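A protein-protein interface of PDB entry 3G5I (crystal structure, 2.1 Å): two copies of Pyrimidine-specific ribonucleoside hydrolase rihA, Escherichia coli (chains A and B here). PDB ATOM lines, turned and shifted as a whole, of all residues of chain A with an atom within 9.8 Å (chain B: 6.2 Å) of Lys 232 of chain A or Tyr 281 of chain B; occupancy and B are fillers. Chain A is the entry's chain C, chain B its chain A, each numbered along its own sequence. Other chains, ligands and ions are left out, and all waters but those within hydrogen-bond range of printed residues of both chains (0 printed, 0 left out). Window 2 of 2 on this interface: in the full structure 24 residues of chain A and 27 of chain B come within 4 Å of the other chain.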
ATOM      1  N   LEU A 157      -5.476 -25.137   7.332  1.00  0.00           N
ATOM      2  CA  LEU A 157      -5.966 -23.819   6.894  1.00  0.00           C
ATOM      3  C   LEU A 157      -6.693 -23.074   8.018  1.00  0.00           C
ATOM      4  O   LEU A 157      -7.353 -23.700   8.869  1.00  0.00           O
ATOM      5  CB  LEU A 157      -6.882 -23.962   5.681  1.00  0.00           C
ATOM      6  CG  LEU A 157      -6.197 -24.393   4.374  1.00  0.00           C
ATOM      7  CD1 LEU A 157      -7.204 -24.807   3.330  1.00  0.00           C
ATOM      8  CD2 LEU A 157      -5.314 -23.323   3.827  1.00  0.00           C
ATOM      9  N   GLY A 158      -6.597 -21.752   8.023  1.00  0.00           N
ATOM     10  CA  GLY A 158      -7.211 -20.954   9.107  1.00  0.00           C
ATOM     11  C   GLY A 158      -8.693 -20.712   8.817  1.00  0.00           C
ATOM     12  O   GLY A 158      -9.143 -20.993   7.702  1.00  0.00           O
ATOM     13  N   ASN A 159      -9.453 -20.235   9.822  1.00  0.00           N
ATOM     14  CA  ASN A 159     -10.853 -19.814   9.557  1.00  0.00           C
ATOM     15  C   ASN A 159     -11.044 -18.298   9.526  1.00  0.00           C
ATOM     16  O   ASN A 159     -12.148 -17.809   9.287  1.00  0.00           O
ATOM     17  CB  ASN A 159     -11.840 -20.490  10.510  1.00  0.00           C
ATOM     18  CG  ASN A 159     -11.660 -20.070  11.954  1.00  0.00           C
ATOM     19  OD1 ASN A 159     -10.747 -19.330  12.281  1.00  0.00           O
ATOM     20  ND2 ASN A 159     -12.556 -20.541  12.832  1.00  0.00           N
ATOM     21  N   TRP A 160      -9.961 -17.548   9.724  1.00  0.00           N
ATOM     22  CA  TRP A 160     -10.087 -16.109   9.840  1.00  0.00           C
ATOM     23  C   TRP A 160      -9.330 -15.377   8.736  1.00  0.00           C
ATOM     24  O   TRP A 160      -9.909 -14.554   8.008  1.00  0.00           O
ATOM     25  CB  TRP A 160      -9.744 -15.598  11.255  1.00  0.00           C
ATOM     26  CG  TRP A 160     -10.210 -14.208  11.441  1.00  0.00           C
ATOM     27  CD1 TRP A 160      -9.456 -13.070  11.429  1.00  0.00           C
ATOM     28  CD2 TRP A 160     -11.582 -13.781  11.542  1.00  0.00           C
ATOM     29  NE1 TRP A 160     -10.277 -11.953  11.544  1.00  0.00           N
ATOM     30  CE2 TRP A 160     -11.580 -12.370  11.645  1.00  0.00           C
ATOM     31  CE3 TRP A 160     -12.809 -14.463  11.580  1.00  0.00           C
ATOM     32  CZ2 TRP A 160     -12.770 -11.621  11.779  1.00  0.00           C
ATOM     33  CZ3 TRP A 160     -14.002 -13.710  11.721  1.00  0.00           C
ATOM     34  CH2 TRP A 160     -13.967 -12.314  11.814  1.00  0.00           C
ATOM     35  N   THR A 161      -8.042 -15.715   8.618  1.00  0.00           N
ATOM     36  CA  THR A 161      -7.219 -15.408   7.431  1.00  0.00           C
ATOM     37  C   THR A 161      -6.820 -16.777   6.844  1.00  0.00           C
ATOM     38  O   THR A 161      -7.102 -17.778   7.457  1.00  0.00           O
ATOM     39  CB  THR A 161      -5.978 -14.657   7.866  1.00  0.00           C
ATOM     40  OG1 THR A 161      -5.298 -15.469   8.837  1.00  0.00           O
ATOM     41  CG2 THR A 161      -6.376 -13.365   8.544  1.00  0.00           C
ATOM     42  N   PRO A 162      -6.248 -16.833   5.619  1.00  0.00           N
ATOM     43  CA  PRO A 162      -5.814 -18.136   5.071  1.00  0.00           C
ATOM     44  C   PRO A 162      -4.972 -18.975   6.034  1.00  0.00           C
ATOM     45  O   PRO A 162      -5.168 -20.196   6.129  1.00  0.00           O
ATOM     46  CB  PRO A 162      -5.004 -17.717   3.828  1.00  0.00           C
ATOM     47  CG  PRO A 162      -5.709 -16.515   3.362  1.00  0.00           C
ATOM     48  CD  PRO A 162      -6.044 -15.755   4.617  1.00  0.00           C
ATOM     49  N   HIS A 194     -13.063 -29.055  13.790  1.00  0.00           N
ATOM     50  CA  HIS A 194     -13.843 -29.138  12.569  1.00  0.00           C
ATOM     51  C   HIS A 194     -14.330 -30.564  12.347  1.00  0.00           C
ATOM     52  O   HIS A 194     -15.224 -30.805  11.513  1.00  0.00           O
ATOM     53  CB  HIS A 194     -13.056 -28.665  11.350  1.00  0.00           C
ATOM     54  CG  HIS A 194     -13.046 -27.170  11.156  1.00  0.00           C
ATOM     55  ND1 HIS A 194     -12.255 -26.550  10.207  1.00  0.00           N
ATOM     56  CD2 HIS A 194     -13.719 -26.181  11.782  1.00  0.00           C
ATOM     57  CE1 HIS A 194     -12.455 -25.244  10.249  1.00  0.00           C
ATOM     58  NE2 HIS A 194     -13.342 -24.992  11.195  1.00  0.00           N
ATOM     59  N   GLU A 231     -20.096 -22.421   4.881  1.00  0.00           N
ATOM     60  CA  GLU A 231     -20.832 -22.973   3.738  1.00  0.00           C
ATOM     61  C   GLU A 231     -19.878 -23.540   2.666  1.00  0.00           C
ATOM     62  O   GLU A 231     -20.168 -24.583   2.049  1.00  0.00           O
ATOM     63  CB  GLU A 231     -21.799 -21.922   3.143  1.00  0.00           C
ATOM     64  CG  GLU A 231     -22.480 -21.019   4.208  1.00  0.00           C
ATOM     65  CD  GLU A 231     -23.798 -20.381   3.754  1.00  0.00           C
ATOM     66  OE1 GLU A 231     -23.988 -20.127   2.532  1.00  0.00           O
ATOM     67  OE2 GLU A 231     -24.645 -20.122   4.646  1.00  0.00           O
ATOM     68  N   LYS A 232     -18.749 -22.843   2.470  1.00  0.00           N
ATOM     69  CA  LYS A 232     -17.656 -23.230   1.541  1.00  0.00           C
ATOM     70  C   LYS A 232     -16.771 -24.334   2.117  1.00  0.00           C
ATOM     71  O   LYS A 232     -16.051 -25.032   1.387  1.00  0.00           O
ATOM     72  CB  LYS A 232     -16.796 -22.006   1.191  1.00  0.00           C
ATOM     73  CG  LYS A 232     -16.491 -21.100   2.385  1.00  0.00           C
ATOM     74  CD  LYS A 232     -16.231 -19.690   1.911  1.00  0.00           C
ATOM     75  CE  LYS A 232     -16.305 -18.716   3.115  1.00  0.00           C
ATOM     76  NZ  LYS A 232     -15.902 -17.343   2.576  1.00  0.00           N
ATOM     77  N   TRP A 233     -16.839 -24.469   3.434  1.00  0.00           N
ATOM     78  CA  TRP A 233     -16.143 -25.525   4.157  1.00  0.00           C
ATOM     79  C   TRP A 233     -16.724 -26.918   3.911  1.00  0.00           C
ATOM     80  O   TRP A 233     -16.017 -27.927   4.040  1.00  0.00           O
ATOM     81  CB  TRP A 233     -16.120 -25.218   5.658  1.00  0.00           C
ATOM     82  CG  TRP A 233     -14.892 -24.441   6.100  1.00  0.00           C
ATOM     83  CD1 TRP A 233     -13.651 -24.960   6.428  1.00  0.00           C
ATOM     84  CD2 TRP A 233     -14.784 -23.017   6.251  1.00  0.00           C
ATOM     85  NE1 TRP A 233     -12.786 -23.940   6.771  1.00  0.00           N
ATOM     86  CE2 TRP A 233     -13.454 -22.741   6.681  1.00  0.00           C
ATOM     87  CE3 TRP A 233     -15.680 -21.944   6.065  1.00  0.00           C
ATOM     88  CZ2 TRP A 233     -12.998 -21.434   6.929  1.00  0.00           C
ATOM     89  CZ3 TRP A 233     -15.220 -20.636   6.318  1.00  0.00           C
ATOM     90  CH2 TRP A 233     -13.885 -20.403   6.746  1.00  0.00           C
ATOM     91  N   GLY A 234     -18.005 -26.965   3.550  1.00  0.00           N
ATOM     92  CA  GLY A 234     -18.712 -28.229   3.296  1.00  0.00           C
ATOM     93  C   GLY A 234     -18.829 -29.121   4.529  1.00  0.00           C
ATOM     94  O   GLY A 234     -18.623 -30.340   4.442  1.00  0.00           O
ATOM     95  N   PHE A 235     -19.130 -28.517   5.680  1.00  0.00           N
ATOM     96  CA  PHE A 235     -19.386 -29.282   6.888  1.00  0.00           C
ATOM     97  C   PHE A 235     -20.750 -29.966   6.741  1.00  0.00           C
ATOM     98  O   PHE A 235     -21.691 -29.407   6.161  1.00  0.00           O
ATOM     99  CB  PHE A 235     -19.402 -28.395   8.141  1.00  0.00           C
ATOM    100  CG  PHE A 235     -18.118 -27.638   8.399  1.00  0.00           C
ATOM    101  CD1 PHE A 235     -16.871 -28.266   8.286  1.00  0.00           C
ATOM    102  CD2 PHE A 235     -18.160 -26.287   8.781  1.00  0.00           C
ATOM    103  CE1 PHE A 235     -15.685 -27.567   8.537  1.00  0.00           C
ATOM    104  CE2 PHE A 235     -16.977 -25.568   9.036  1.00  0.00           C
ATOM    105  CZ  PHE A 235     -15.741 -26.217   8.919  1.00  0.00           C
ATOM    106  N   VAL A 236     -20.841 -31.179   7.280  1.00  0.00           N
ATOM    107  CA  VAL A 236     -22.097 -31.914   7.395  1.00  0.00           C
ATOM    108  C   VAL A 236     -23.004 -31.334   8.495  1.00  0.00           C
ATOM    109  O   VAL A 236     -24.204 -31.272   8.340  1.00  0.00           O
ATOM    110  CB  VAL A 236     -21.829 -33.418   7.625  1.00  0.00           C
ATOM    111  CG1 VAL A 236     -23.115 -34.195   7.914  1.00  0.00           C
ATOM    112  CG2 VAL A 236     -21.108 -34.015   6.423  1.00  0.00           C
ATOM    113  N   GLU B 259      -8.850 -22.082  -8.690  1.00  0.00           N
ATOM    114  CA  GLU B 259      -8.280 -20.776  -8.926  1.00  0.00           C
ATOM    115  C   GLU B 259      -8.427 -19.969  -7.667  1.00  0.00           C
ATOM    116  O   GLU B 259      -9.541 -19.653  -7.231  1.00  0.00           O
ATOM    117  CB  GLU B 259      -8.987 -20.056 -10.063  1.00  0.00           C
ATOM    118  CG  GLU B 259      -8.580 -20.509 -11.436  1.00  0.00           C
ATOM    119  CD  GLU B 259      -9.649 -20.153 -12.462  1.00  0.00           C
ATOM    120  OE1 GLU B 259     -10.525 -19.326 -12.137  1.00  0.00           O
ATOM    121  OE2 GLU B 259      -9.638 -20.696 -13.575  1.00  0.00           O
ATOM    122  N   ARG B 260      -7.284 -19.641  -7.061  1.00  0.00           N
ATOM    123  CA  ARG B 260      -7.298 -18.919  -5.777  1.00  0.00           C
ATOM    124  C   ARG B 260      -6.195 -17.872  -5.734  1.00  0.00           C
ATOM    125  O   ARG B 260      -5.287 -17.895  -6.560  1.00  0.00           O
ATOM    126  CB  ARG B 260      -7.146 -19.906  -4.602  1.00  0.00           C
ATOM    127  CG  ARG B 260      -8.268 -20.894  -4.444  1.00  0.00           C
ATOM    128  CD  ARG B 260      -9.602 -20.237  -4.093  1.00  0.00           C
ATOM    129  NE  ARG B 260     -10.592 -21.256  -3.749  1.00  0.00           N
ATOM    130  CZ  ARG B 260     -11.332 -21.922  -4.622  1.00  0.00           C
ATOM    131  NH1 ARG B 260     -11.259 -21.656  -5.928  1.00  0.00           N
ATOM    132  NH2 ARG B 260     -12.189 -22.831  -4.171  1.00  0.00           N
ATOM    133  N   TRP B 261      -6.255 -16.971  -4.749  1.00  0.00           N
ATOM    134  CA  TRP B 261      -5.132 -16.068  -4.483  1.00  0.00           C
ATOM    135  C   TRP B 261      -4.078 -16.835  -3.729  1.00  0.00           C
ATOM    136  O   TRP B 261      -4.407 -17.613  -2.783  1.00  0.00           O
ATOM    137  CB  TRP B 261      -5.573 -14.873  -3.654  1.00  0.00           C
ATOM    138  CG  TRP B 261      -4.479 -13.975  -3.378  1.00  0.00           C
ATOM    139  CD1 TRP B 261      -3.870 -13.084  -4.261  1.00  0.00           C
ATOM    140  CD2 TRP B 261      -3.763 -13.884  -2.140  1.00  0.00           C
ATOM    141  NE1 TRP B 261      -2.825 -12.441  -3.605  1.00  0.00           N
ATOM    142  CE2 TRP B 261      -2.718 -12.945  -2.326  1.00  0.00           C
ATOM    143  CE3 TRP B 261      -3.867 -14.558  -0.908  1.00  0.00           C
ATOM    144  CZ2 TRP B 261      -1.840 -12.609  -1.310  1.00  0.00           C
ATOM    145  CZ3 TRP B 261      -2.970 -14.236   0.107  1.00  0.00           C
ATOM    146  CH2 TRP B 261      -1.969 -13.278  -0.103  1.00  0.00           C
ATOM    147  N   ASP B 278      -5.494 -18.691  -0.428  1.00  0.00           N
ATOM    148  CA  ASP B 278      -6.746 -18.222   0.132  1.00  0.00           C
ATOM    149  C   ASP B 278      -7.860 -19.120  -0.364  1.00  0.00           C
ATOM    150  O   ASP B 278      -8.695 -18.731  -1.173  1.00  0.00           O
ATOM    151  CB  ASP B 278      -7.001 -16.752  -0.154  1.00  0.00           C
ATOM    152  CG  ASP B 278      -8.242 -16.252   0.543  1.00  0.00           C
ATOM    153  OD1 ASP B 278      -8.738 -16.947   1.484  1.00  0.00           O
ATOM    154  OD2 ASP B 278      -8.787 -15.197   0.117  1.00  0.00           O
ATOM    155  N   TYR B 279      -7.848 -20.342   0.157  1.00  0.00           N
ATOM    156  CA  TYR B 279      -8.726 -21.403  -0.321  1.00  0.00           C
ATOM    157  C   TYR B 279     -10.196 -21.166  -0.062  1.00  0.00           C
ATOM    158  O   TYR B 279     -11.035 -21.579  -0.886  1.00  0.00           O
ATOM    159  CB  TYR B 279      -8.322 -22.745   0.279  1.00  0.00           C
ATOM    160  CG  TYR B 279      -9.126 -23.906  -0.299  1.00  0.00           C
ATOM    161  CD1 TYR B 279      -8.711 -24.560  -1.469  1.00  0.00           C
ATOM    162  CD2 TYR B 279     -10.290 -24.344   0.317  1.00  0.00           C
ATOM    163  CE1 TYR B 279      -9.445 -25.624  -1.992  1.00  0.00           C
ATOM    164  CE2 TYR B 279     -11.024 -25.394  -0.199  1.00  0.00           C
ATOM    165  CZ  TYR B 279     -10.605 -26.023  -1.325  1.00  0.00           C
ATOM    166  OH  TYR B 279     -11.356 -27.037  -1.820  1.00  0.00           O
ATOM    167  N   TYR B 280     -10.502 -20.487   1.050  1.00  0.00           N
ATOM    168  CA  TYR B 280     -11.903 -20.185   1.402  1.00  0.00           C
ATOM    169  C   TYR B 280     -12.355 -18.766   1.180  1.00  0.00           C
ATOM    170  O   TYR B 280     -13.370 -18.389   1.754  1.00  0.00           O
ATOM    171  CB  TYR B 280     -12.185 -20.545   2.860  1.00  0.00           C
ATOM    172  CG  TYR B 280     -12.033 -22.008   3.111  1.00  0.00           C
ATOM    173  CD1 TYR B 280     -13.051 -22.904   2.762  1.00  0.00           C
ATOM    174  CD2 TYR B 280     -10.872 -22.511   3.679  1.00  0.00           C
ATOM    175  CE1 TYR B 280     -12.902 -24.269   2.979  1.00  0.00           C
ATOM    176  CE2 TYR B 280     -10.710 -23.849   3.907  1.00  0.00           C
ATOM    177  CZ  TYR B 280     -11.714 -24.731   3.556  1.00  0.00           C
ATOM    178  OH  TYR B 280     -11.527 -26.076   3.792  1.00  0.00           O
ATOM    179  N   TYR B 281     -11.607 -18.000   0.372  1.00  0.00           N
ATOM    180  CA  TYR B 281     -11.941 -16.622   0.015  1.00  0.00           C
ATOM    181  C   TYR B 281     -12.124 -15.696   1.216  1.00  0.00           C
ATOM    182  O   TYR B 281     -13.160 -15.066   1.380  1.00  0.00           O
ATOM    183  CB  TYR B 281     -13.210 -16.610  -0.833  1.00  0.00           C
ATOM    184  CG  TYR B 281     -13.119 -17.383  -2.118  1.00  0.00           C
ATOM    185  CD1 TYR B 281     -12.369 -16.908  -3.186  1.00  0.00           C
ATOM    186  CD2 TYR B 281     -13.824 -18.568  -2.284  1.00  0.00           C
ATOM    187  CE1 TYR B 281     -12.324 -17.624  -4.419  1.00  0.00           C
ATOM    188  CE2 TYR B 281     -13.806 -19.266  -3.483  1.00  0.00           C
ATOM    189  CZ  TYR B 281     -13.055 -18.798  -4.532  1.00  0.00           C
ATOM    190  OH  TYR B 281     -13.017 -19.501  -5.703  1.00  0.00           O
ATOM    191  N   LEU B 282     -11.104 -15.603   2.049  1.00  0.00           N
ATOM    192  CA  LEU B 282     -11.222 -14.797   3.243  1.00  0.00           C
ATOM    193  C   LEU B 282     -10.603 -13.437   3.039  1.00  0.00           C
ATOM    194  O   LEU B 282     -10.888 -12.514   3.810  1.00  0.00           O
ATOM    195  CB  LEU B 282     -10.557 -15.498   4.449  1.00  0.00           C
ATOM    196  CG  LEU B 282     -11.086 -16.892   4.809  1.00  0.00           C
ATOM    197  CD1 LEU B 282     -10.165 -17.582   5.819  1.00  0.00           C
ATOM    198  CD2 LEU B 282     -12.517 -16.895   5.272  1.00  0.00           C
ATOM    199  N   THR B 283      -9.740 -13.317   2.031  1.00  0.00           N
ATOM    200  CA  THR B 283      -9.021 -12.059   1.777  1.00  0.00           C
ATOM    201  C   THR B 283      -9.784 -11.232   0.743  1.00  0.00           C
ATOM    202  O   THR B 283     -10.729 -11.717   0.123  1.00  0.00           O
ATOM    203  CB  THR B 283      -7.634 -12.320   1.210  1.00  0.00           C
ATOM    204  OG1 THR B 283      -7.750 -12.842  -0.105  1.00  0.00           O
ATOM    205  CG2 THR B 283      -6.837 -13.346   2.079  1.00  0.00           C
ATOM    206  N   ASN B 285      -8.451 -10.587  -2.022  1.00  0.00           N
ATOM    207  CA  ASN B 285      -7.476 -10.630  -3.103  1.00  0.00           C
ATOM    208  C   ASN B 285      -7.963 -11.379  -4.311  1.00  0.00           C
ATOM    209  O   ASN B 285      -8.589 -12.445  -4.187  1.00  0.00           O
ATOM    210  CB  ASN B 285      -6.154 -11.225  -2.613  1.00  0.00           C
ATOM    211  CG  ASN B 285      -5.581 -10.464  -1.448  1.00  0.00           C
ATOM    212  OD1 ASN B 285      -5.909  -9.293  -1.256  1.00  0.00           O
ATOM    213  ND2 ASN B 285      -4.745 -11.113  -0.643  1.00  0.00           N
ATOM    214  N   PRO B 287      -7.762 -13.777  -7.262  1.00  0.00           N
ATOM    215  CA  PRO B 287      -7.003 -14.960  -7.594  1.00  0.00           C
ATOM    216  C   PRO B 287      -5.887 -14.649  -8.596  1.00  0.00           C
ATOM    217  O   PRO B 287      -6.101 -13.902  -9.543  1.00  0.00           O
ATOM    218  CB  PRO B 287      -8.046 -15.896  -8.207  1.00  0.00           C
ATOM    219  CG  PRO B 287      -9.339 -15.497  -7.536  1.00  0.00           C
ATOM    220  CD  PRO B 287      -9.228 -14.020  -7.266  1.00  0.00           C
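Printed residues of chain B within 4 Å of Thr 161 of chain A: Leu 282. Lys 232 of chain A touches two residues of chain B. Of the printed residues of chain A, Tyr 279 of chain B touches Leu 157. Tyr 281 of chain B touches just one residue of chain A: Lys 232. Printed residues of chain A within 4 Å of Leu 282 of chain B: Asn 159, Trp 160, Thr 161 and Pro 162. Of the printed residues of chain A, Thr 283 of chain B touches Pro 162 (3.6 Å). Asn 285 of chain B touches none of the printed residues of chain A. The nearest residue of chain B that does not touch Lys 232 of chain A is Leu 282 of chain B (4.4 Å). The nearest residue of chain A that does not touch Tyr 281 of chain B is Pro 162 of chain A (6.8 Å).
Of the 11 printed residues of chain B, 6 touch a printed residue of chain A. Printed residues of chain B that touch a printed residue of chain A: Asp 278, Tyr 279, Tyr 280, Tyr 281, Leu 282 and Thr 283. Hydrophobic or aromatic side chains of chain B that line the printed part of chain A: Tyr 279, Tyr 280 and Leu 282. Hydrophobic or aromatic side chains of chain A that line the printed part of chain B: Leu 157, Pro 162 and Trp 233. Along chain A the printed residues that touch a printed residue of chain B span positions 157 to 233. Among the printed residues, 11 pairs touch across the chains. Among the printed residues, no Asp or Glu carboxylate lies within 4 Å of a Lys or Arg side-chain nitrogen of the other chain.
The backbone carbonyl oxygen (O) of Tyr 279 of chain B is in hydrogen-bond range of the guanidinium group (NE) of Arg 260 of chain B, at 2.9 Å. The guanidinium group (NH1) of Arg 260 of chain B is in hydrogen-bond range of the side-chain hydroxyl (OH) of Tyr 281 of chain B (2.8 Å). OD1 of Asp 278 of chain B sits at hydrogen-bond distance from N of Tyr 281 of chain B, at 3.3 Å. OD1 of Asp 278 of chain B sits at hydrogen-bond distance from N of Leu 282 of chain B (2.8 Å). OD2 of Asp 278 of chain B sits at hydrogen-bond distance from OG1 of Thr 283 of chain B, 2.6 Å away. OG1 of Thr 283 of chain B is in hydrogen-bond range of N of Asn 285 of chain B, 3.0 Å away.
No position is printed for both chains. Of the 11 pairs that touch across the chains among the printed residues, none has its exchanged pair printed and touching as well.
The backbone carbonyl oxygen (O) of Tyr 280 of chain B lies within hydrogen-bond range of the side-chain amino group (NZ) of Lys 232 of chain A, at 2.9 Å.
CB of Tyr 279 of chain B touches CD1 of Leu 157 of chain A (3.8 Å). Leu 157 of chain A touches Tyr 280 of chain B (CD1 to CE2, 3.7 Å). C of Asn 159 of chain A touches CD1 of Leu 282 of chain B, at 3.9 Å. Trp 160 of chain A touches Leu 282 of chain B. O of Thr 161 of chain A touches CD1 of Leu 282 of chain B (3.5 Å). Pro 162 of chain A touches Asp 278 of chain B (CG to OD1, 3.6 Å). N of Pro 162 of chain A touches CD1 of Leu 282 of chain B, 3.99 Å away. CG2 of Thr 283 of chain B touches CD of Pro 162 of chain A, at 3.6 Å. Tyr 281 of chain B touches Lys 232 of chain A (O to NZ, 3.8 Å). Trp 233 of chain A touches Tyr 280 of chain B (CD1 to CZ, 3.5 Å).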
